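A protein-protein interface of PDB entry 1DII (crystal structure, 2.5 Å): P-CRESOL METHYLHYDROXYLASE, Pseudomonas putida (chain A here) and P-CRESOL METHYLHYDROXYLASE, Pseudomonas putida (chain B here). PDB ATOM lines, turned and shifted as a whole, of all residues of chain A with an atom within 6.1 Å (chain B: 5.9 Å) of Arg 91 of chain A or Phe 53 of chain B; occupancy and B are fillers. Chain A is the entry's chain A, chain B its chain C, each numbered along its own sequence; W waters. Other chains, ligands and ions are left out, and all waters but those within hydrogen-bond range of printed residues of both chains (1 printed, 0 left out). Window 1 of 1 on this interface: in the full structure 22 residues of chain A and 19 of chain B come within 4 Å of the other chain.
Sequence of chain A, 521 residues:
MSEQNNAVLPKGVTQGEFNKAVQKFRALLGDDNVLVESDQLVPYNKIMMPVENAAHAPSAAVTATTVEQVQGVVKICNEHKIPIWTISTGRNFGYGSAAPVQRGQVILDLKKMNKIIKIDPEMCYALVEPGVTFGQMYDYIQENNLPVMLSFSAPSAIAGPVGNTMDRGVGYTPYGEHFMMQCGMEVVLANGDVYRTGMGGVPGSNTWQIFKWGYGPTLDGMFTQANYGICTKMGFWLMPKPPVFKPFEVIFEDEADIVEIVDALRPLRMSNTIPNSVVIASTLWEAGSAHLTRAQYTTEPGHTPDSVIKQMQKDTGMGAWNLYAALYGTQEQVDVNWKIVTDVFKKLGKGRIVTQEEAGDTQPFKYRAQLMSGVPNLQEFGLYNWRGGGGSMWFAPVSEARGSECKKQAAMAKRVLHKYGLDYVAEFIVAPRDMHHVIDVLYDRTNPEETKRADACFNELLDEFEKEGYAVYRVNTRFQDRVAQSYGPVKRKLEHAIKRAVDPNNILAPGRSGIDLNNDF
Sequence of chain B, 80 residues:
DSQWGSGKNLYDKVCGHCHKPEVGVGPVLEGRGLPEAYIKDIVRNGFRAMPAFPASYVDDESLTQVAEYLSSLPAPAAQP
The side-chain hydroxyl (OH) of Tyr 57 of chain B is in hydrogen-bond range of the backbone carbonyl oxygen (O) of Ile 158 of chain A (2.7 Å). NH1 of Arg 91 of chain A is in hydrogen-bond range of O of Ala 52 of chain B. N of Pro 43 of chain A sits close to O of Arg 44 of chain B (3.3 Å).
The backbone carbonyl oxygen (O) of Thr 89 of chain A lies within hydrogen-bond range of the guanidinium group (NE) of Arg 91 of chain A, 3.1 Å away. The backbone carbonyl oxygen (O) of Phe 53 of chain B is in hydrogen-bond range of the guanidinium group (NH1) of Arg 44 of chain B, at 3.3 Å. O of Val 43 of chain B is in hydrogen-bond range of N of Phe 53 of chain B (3.0 Å). O of Val 58 of chain B lies within hydrogen-bond range of NH1 of Arg 44 of chain B (2.8 Å).
Among the printed residues, pairs that only touch across the chains: Pro 43 of chain A with Ala 52 of chain B, Pro 43 of chain A with Phe 53 of chain B, Pro 43 of chain A with Pro 54 of chain B, Arg 91 of chain A with Phe 53 of chain B, Arg 91 of chain A with Pro 54 of chain B and Phe 93 of chain A with Pro 51 of chain B.
Of chain B, only Ala 52, Phe 53 and Pro 54 come within 4 Å of Arg 91 of chain A. Of chain A, only Pro 43 (3.7 Å) and Arg 91 (3.9 Å) come within 4 Å of Phe 53 of chain B. Printed residues of chain B within 4 Å of Phe 93 of chain A: Pro 51. Printed residues of chain A within 4 Å of Ala 52 of chain B: Pro 43 (3.4 Å) and Arg 91 (2.7 Å). Of the printed residues of chain B, Ile 158 of chain A touches Tyr 57 (2.7 Å). Printed residues of chain A within 4 Å of Pro 51 of chain B: Phe 93. Ala 159 of chain A touches none of the printed residues of chain B. Ser 97 of chain A touches none of the printed residues of chain B. The nearest residue of chain A that does not touch Phe 53 of chain B is Ile 158 of chain A (4.4 Å). The nearest printed residue of chain A that does not touch Ala 52 of chain B is Phe 93 of chain A (5.6 Å).
Of the 12 printed residues of chain A, 4 touch a printed residue of chain B. Printed residues of chain A that touch a printed residue of chain B: Pro 43, Arg 91, Phe 93 and Ile 158. Printed residues of chain B that touch a printed residue of chain A: Arg 44, Pro 51, Ala 52, Phe 53, Pro 54 and Tyr 57. Among the printed residues, 9 pairs touch across the chains.
Water W1 lies within hydrogen-bond range of O of Pro 43 of chain A, NH2 of Arg 91 of chain A and O of Ala 52 of chain B.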
ATOM      1  N   PRO A  43      -7.063  25.370 -29.651  1.00  0.00           N
ATOM      2  CA  PRO A  43      -6.752  24.004 -29.193  1.00  0.00           C
ATOM      3  C   PRO A  43      -6.170  23.837 -27.781  1.00  0.00           C
ATOM      4  O   PRO A  43      -6.125  22.734 -27.249  1.00  0.00           O
ATOM      5  CB  PRO A  43      -5.798  23.481 -30.275  1.00  0.00           C
ATOM      6  CG  PRO A  43      -5.234  24.688 -30.879  1.00  0.00           C
ATOM      7  CD  PRO A  43      -6.366  25.624 -30.930  1.00  0.00           C
ATOM      8  N   THR A  89       4.066  18.669 -22.718  1.00  0.00           N
ATOM      9  CA  THR A  89       3.323  17.941 -23.756  1.00  0.00           C
ATOM     10  C   THR A  89       1.832  18.318 -23.665  1.00  0.00           C
ATOM     11  O   THR A  89       1.086  18.131 -24.622  1.00  0.00           O
ATOM     12  CB  THR A  89       3.540  16.403 -23.708  1.00  0.00           C
ATOM     13  OG1 THR A  89       3.596  15.959 -22.356  1.00  0.00           O
ATOM     14  CG2 THR A  89       4.816  16.020 -24.399  1.00  0.00           C
ATOM     15  N   GLY A  90       1.438  18.903 -22.528  1.00  0.00           N
ATOM     16  CA  GLY A  90       0.085  19.402 -22.280  1.00  0.00           C
ATOM     17  C   GLY A  90      -1.100  18.465 -22.399  1.00  0.00           C
ATOM     18  O   GLY A  90      -2.214  18.918 -22.689  1.00  0.00           O
ATOM     19  N   ARG A  91      -0.870  17.173 -22.164  1.00  0.00           N
ATOM     20  CA  ARG A  91      -1.914  16.159 -22.265  1.00  0.00           C
ATOM     21  C   ARG A  91      -2.488  15.797 -20.889  1.00  0.00           C
ATOM     22  O   ARG A  91      -2.825  14.645 -20.639  1.00  0.00           O
ATOM     23  CB  ARG A  91      -1.353  14.899 -22.952  1.00  0.00           C
ATOM     24  CG  ARG A  91      -0.633  15.103 -24.291  1.00  0.00           C
ATOM     25  CD  ARG A  91      -1.530  15.600 -25.434  1.00  0.00           C
ATOM     26  NE  ARG A  91      -1.771  17.041 -25.370  1.00  0.00           N
ATOM     27  CZ  ARG A  91      -2.736  17.679 -26.028  1.00  0.00           C
ATOM     28  NH1 ARG A  91      -3.568  17.006 -26.822  1.00  0.00           N
ATOM     29  NH2 ARG A  91      -2.902  18.986 -25.844  1.00  0.00           N
ATOM     30  N   ASN A  92      -2.695  16.801 -20.042  1.00  0.00           N
ATOM     31  CA  ASN A  92      -3.188  16.604 -18.678  1.00  0.00           C
ATOM     32  C   ASN A  92      -4.704  16.453 -18.522  1.00  0.00           C
ATOM     33  O   ASN A  92      -5.334  17.168 -17.713  1.00  0.00           O
ATOM     34  CB  ASN A  92      -2.646  17.749 -17.807  1.00  0.00           C
ATOM     35  CG  ASN A  92      -2.257  17.314 -16.404  1.00  0.00           C
ATOM     36  OD1 ASN A  92      -2.147  16.107 -16.082  1.00  0.00           O
ATOM     37  ND2 ASN A  92      -2.058  18.316 -15.538  1.00  0.00           N
ATOM     38  N   PHE A  93      -5.265  15.482 -19.256  1.00  0.00           N
ATOM     39  CA  PHE A  93      -6.697  15.171 -19.278  1.00  0.00           C
ATOM     40  C   PHE A  93      -7.285  14.799 -17.925  1.00  0.00           C
ATOM     41  O   PHE A  93      -6.833  13.851 -17.275  1.00  0.00           O
ATOM     42  CB  PHE A  93      -6.980  14.038 -20.261  1.00  0.00           C
ATOM     43  CG  PHE A  93      -6.389  14.251 -21.616  1.00  0.00           C
ATOM     44  CD1 PHE A  93      -6.613  15.445 -22.319  1.00  0.00           C
ATOM     45  CD2 PHE A  93      -5.548  13.275 -22.175  1.00  0.00           C
ATOM     46  CE1 PHE A  93      -5.992  15.654 -23.553  1.00  0.00           C
ATOM     47  CE2 PHE A  93      -4.924  13.471 -23.411  1.00  0.00           C
ATOM     48  CZ  PHE A  93      -5.141  14.654 -24.100  1.00  0.00           C
ATOM     49  N   SER A  97      -5.922  19.903 -18.591  1.00  0.00           N
ATOM     50  CA  SER A  97      -5.412  19.788 -19.953  1.00  0.00           C
ATOM     51  C   SER A  97      -4.226  20.744 -20.183  1.00  0.00           C
ATOM     52  O   SER A  97      -3.281  20.739 -19.383  1.00  0.00           O
ATOM     53  CB  SER A  97      -6.536  19.922 -20.992  1.00  0.00           C
ATOM     54  OG  SER A  97      -7.355  18.760 -20.998  1.00  0.00           O
ATOM     55  N   ALA A  98      -4.279  21.558 -21.235  1.00  0.00           N
ATOM     56  CA  ALA A  98      -3.206  22.489 -21.547  1.00  0.00           C
ATOM     57  C   ALA A  98      -3.588  23.925 -21.195  1.00  0.00           C
ATOM     58  O   ALA A  98      -2.779  24.844 -21.360  1.00  0.00           O
ATOM     59  CB  ALA A  98      -2.879  22.395 -23.014  1.00  0.00           C
ATOM     60  N   PRO A 155      -2.099   7.664 -21.283  1.00  0.00           N
ATOM     61  CA  PRO A 155      -1.829   8.614 -22.377  1.00  0.00           C
ATOM     62  C   PRO A 155      -0.561   8.297 -23.153  1.00  0.00           C
ATOM     63  O   PRO A 155      -0.393   8.737 -24.295  1.00  0.00           O
ATOM     64  CB  PRO A 155      -1.691   9.933 -21.642  1.00  0.00           C
ATOM     65  CG  PRO A 155      -2.626   9.785 -20.564  1.00  0.00           C
ATOM     66  CD  PRO A 155      -2.339   8.428 -20.046  1.00  0.00           C
ATOM     67  N   ILE A 158       1.295   9.788 -26.536  1.00  0.00           N
ATOM     68  CA  ILE A 158       1.138  11.215 -26.744  1.00  0.00           C
ATOM     69  C   ILE A 158       1.571  12.113 -25.597  1.00  0.00           C
ATOM     70  O   ILE A 158       1.667  13.327 -25.772  1.00  0.00           O
ATOM     71  CB  ILE A 158      -0.312  11.595 -27.202  1.00  0.00           C
ATOM     72  CG1 ILE A 158      -1.357  11.251 -26.132  1.00  0.00           C
ATOM     73  CG2 ILE A 158      -0.614  10.943 -28.556  1.00  0.00           C
ATOM     74  CD1 ILE A 158      -2.701  11.965 -26.319  1.00  0.00           C
ATOM     75  N   ALA A 159       1.842  11.511 -24.434  1.00  0.00           N
ATOM     76  CA  ALA A 159       2.260  12.250 -23.252  1.00  0.00           C
ATOM     77  C   ALA A 159       3.770  12.219 -23.071  1.00  0.00           C
ATOM     78  O   ALA A 159       4.460  11.476 -23.759  1.00  0.00           O
ATOM     79  CB  ALA A 159       1.555  11.703 -22.015  1.00  0.00           C
ATOM     80  N   GLY A 160       4.272  12.964 -22.088  1.00  0.00           N
ATOM     81  CA  GLY A 160       5.698  12.996 -21.856  1.00  0.00           C
ATOM     82  C   GLY A 160       6.212  12.848 -20.436  1.00  0.00           C
ATOM     83  O   GLY A 160       5.464  13.053 -19.483  1.00  0.00           O
ATOM     84  N   VAL B  14       0.360   8.932 -33.804  1.00  0.00           N
ATOM     85  CA  VAL B  14      -0.646   9.622 -32.992  1.00  0.00           C
ATOM     86  C   VAL B  14      -2.074   9.107 -33.174  1.00  0.00           C
ATOM     87  O   VAL B  14      -2.569   8.352 -32.336  1.00  0.00           O
ATOM     88  CB  VAL B  14      -0.609  11.167 -33.211  1.00  0.00           C
ATOM     89  CG1 VAL B  14      -1.630  11.894 -32.313  1.00  0.00           C
ATOM     90  CG2 VAL B  14       0.756  11.683 -32.937  1.00  0.00           C
ATOM     91  N   VAL B  43      -9.220  18.444 -35.228  1.00  0.00           N
ATOM     92  CA  VAL B  43      -7.922  18.402 -34.545  1.00  0.00           C
ATOM     93  C   VAL B  43      -7.620  19.698 -33.772  1.00  0.00           C
ATOM     94  O   VAL B  43      -7.157  19.643 -32.641  1.00  0.00           O
ATOM     95  CB  VAL B  43      -6.786  18.007 -35.509  1.00  0.00           C
ATOM     96  CG1 VAL B  43      -5.436  18.063 -34.831  1.00  0.00           C
ATOM     97  CG2 VAL B  43      -6.997  16.598 -35.966  1.00  0.00           C
ATOM     98  N   ARG B  44      -7.949  20.846 -34.344  1.00  0.00           N
ATOM     99  CA  ARG B  44      -7.716  22.119 -33.668  1.00  0.00           C
ATOM    100  C   ARG B  44      -8.748  22.459 -32.583  1.00  0.00           C
ATOM    101  O   ARG B  44      -8.448  23.210 -31.670  1.00  0.00           O
ATOM    102  CB  ARG B  44      -7.648  23.281 -34.679  1.00  0.00           C
ATOM    103  CG  ARG B  44      -6.463  23.237 -35.635  1.00  0.00           C
ATOM    104  CD  ARG B  44      -5.150  23.505 -34.930  1.00  0.00           C
ATOM    105  NE  ARG B  44      -4.042  23.520 -35.870  1.00  0.00           N
ATOM    106  CZ  ARG B  44      -3.177  22.529 -36.053  1.00  0.00           C
ATOM    107  NH1 ARG B  44      -3.263  21.392 -35.362  1.00  0.00           N
ATOM    108  NH2 ARG B  44      -2.194  22.693 -36.923  1.00  0.00           N
ATOM    109  N   GLY B  46     -10.941  19.943 -31.205  1.00  0.00           N
ATOM    110  CA  GLY B  46     -11.161  18.760 -30.400  1.00  0.00           C
ATOM    111  C   GLY B  46     -12.648  18.491 -30.567  1.00  0.00           C
ATOM    112  O   GLY B  46     -13.385  19.371 -31.012  1.00  0.00           O
ATOM    113  N   MET B  50     -12.702  13.333 -27.954  1.00  0.00           N
ATOM    114  CA  MET B  50     -11.436  13.546 -28.641  1.00  0.00           C
ATOM    115  C   MET B  50     -10.722  14.821 -28.200  1.00  0.00           C
ATOM    116  O   MET B  50     -11.342  15.884 -28.153  1.00  0.00           O
ATOM    117  CB  MET B  50     -11.622  13.645 -30.169  1.00  0.00           C
ATOM    118  CG  MET B  50     -10.262  13.733 -30.875  1.00  0.00           C
ATOM    119  SD  MET B  50     -10.116  13.608 -32.583  1.00  0.00           S
ATOM    120  CE  MET B  50      -8.817  14.715 -32.781  1.00  0.00           C
ATOM    121  N   PRO B  51      -9.409  14.719 -27.881  1.00  0.00           N
ATOM    122  CA  PRO B  51      -8.668  15.912 -27.475  1.00  0.00           C
ATOM    123  C   PRO B  51      -8.239  16.778 -28.663  1.00  0.00           C
ATOM    124  O   PRO B  51      -8.364  16.387 -29.826  1.00  0.00           O
ATOM    125  CB  PRO B  51      -7.464  15.330 -26.756  1.00  0.00           C
ATOM    126  CG  PRO B  51      -7.284  13.970 -27.341  1.00  0.00           C
ATOM    127  CD  PRO B  51      -8.670  13.491 -27.499  1.00  0.00           C
ATOM    128  N   ALA B  52      -7.781  17.975 -28.343  1.00  0.00           N
ATOM    129  CA  ALA B  52      -7.287  18.916 -29.329  1.00  0.00           C
ATOM    130  C   ALA B  52      -5.769  18.887 -29.348  1.00  0.00           C
ATOM    131  O   ALA B  52      -5.146  18.690 -28.308  1.00  0.00           O
ATOM    132  CB  ALA B  52      -7.744  20.291 -28.981  1.00  0.00           C
ATOM    133  N   PHE B  53      -5.181  19.038 -30.530  1.00  0.00           N
ATOM    134  CA  PHE B  53      -3.728  19.095 -30.674  1.00  0.00           C
ATOM    135  C   PHE B  53      -3.342  20.486 -31.205  1.00  0.00           C
ATOM    136  O   PHE B  53      -3.912  20.955 -32.202  1.00  0.00           O
ATOM    137  CB  PHE B  53      -3.216  18.012 -31.625  1.00  0.00           C
ATOM    138  CG  PHE B  53      -3.420  16.609 -31.119  1.00  0.00           C
ATOM    139  CD1 PHE B  53      -4.634  15.936 -31.331  1.00  0.00           C
ATOM    140  CD2 PHE B  53      -2.413  15.961 -30.401  1.00  0.00           C
ATOM    141  CE1 PHE B  53      -4.850  14.617 -30.821  1.00  0.00           C
ATOM    142  CE2 PHE B  53      -2.615  14.644 -29.887  1.00  0.00           C
ATOM    143  CZ  PHE B  53      -3.840  13.977 -30.099  1.00  0.00           C
ATOM    144  N   PRO B  54      -2.460  21.219 -30.486  1.00  0.00           N
ATOM    145  CA  PRO B  54      -2.053  22.546 -30.974  1.00  0.00           C
ATOM    146  C   PRO B  54      -1.091  22.390 -32.164  1.00  0.00           C
ATOM    147  O   PRO B  54      -0.581  21.278 -32.417  1.00  0.00           O
ATOM    148  CB  PRO B  54      -1.355  23.165 -29.761  1.00  0.00           C
ATOM    149  CG  PRO B  54      -1.974  22.482 -28.618  1.00  0.00           C
ATOM    150  CD  PRO B  54      -2.020  21.047 -29.091  1.00  0.00           C
ATOM    151  N   ALA B  55      -0.857  23.490 -32.884  1.00  0.00           N
ATOM    152  CA  ALA B  55       0.026  23.510 -34.057  1.00  0.00           C
ATOM    153  C   ALA B  55       1.457  23.029 -33.745  1.00  0.00           C
ATOM    154  O   ALA B  55       2.077  22.329 -34.563  1.00  0.00           O
ATOM    155  CB  ALA B  55       0.036  24.904 -34.684  1.00  0.00           C
ATOM    156  N   TYR B  57       2.240  20.690 -31.755  1.00  0.00           N
ATOM    157  CA  TYR B  57       2.206  19.235 -31.692  1.00  0.00           C
ATOM    158  C   TYR B  57       2.025  18.636 -33.100  1.00  0.00           C
ATOM    159  O   TYR B  57       2.757  17.719 -33.484  1.00  0.00           O
ATOM    160  CB  TYR B  57       1.076  18.760 -30.746  1.00  0.00           C
ATOM    161  CG  TYR B  57       1.300  17.399 -30.097  1.00  0.00           C
ATOM    162  CD1 TYR B  57       1.500  16.231 -30.887  1.00  0.00           C
ATOM    163  CD2 TYR B  57       1.344  17.267 -28.688  1.00  0.00           C
ATOM    164  CE1 TYR B  57       1.749  14.965 -30.307  1.00  0.00           C
ATOM    165  CE2 TYR B  57       1.584  15.994 -28.079  1.00  0.00           C
ATOM    166  CZ  TYR B  57       1.789  14.858 -28.915  1.00  0.00           C
ATOM    167  OH  TYR B  57       2.057  13.634 -28.390  1.00  0.00           O
ATOM    168  N   VAL B  58       0.976  19.082 -33.794  1.00  0.00           N
ATOM    169  CA  VAL B  58       0.644  18.628 -35.153  1.00  0.00           C
ATOM    170  C   VAL B  58       0.370  19.890 -35.990  1.00  0.00           C
ATOM    171  O   VAL B  58      -0.717  20.468 -35.876  1.00  0.00           O
ATOM    172  CB  VAL B  58      -0.657  17.721 -35.185  1.00  0.00           C
ATOM    173  CG1 VAL B  58      -0.917  17.232 -36.573  1.00  0.00           C
ATOM    174  CG2 VAL B  58      -0.550  16.517 -34.259  1.00  0.00           C
HETATM  175  O   HOH W   1      -5.356  20.955 -25.750  1.00  0.00           O
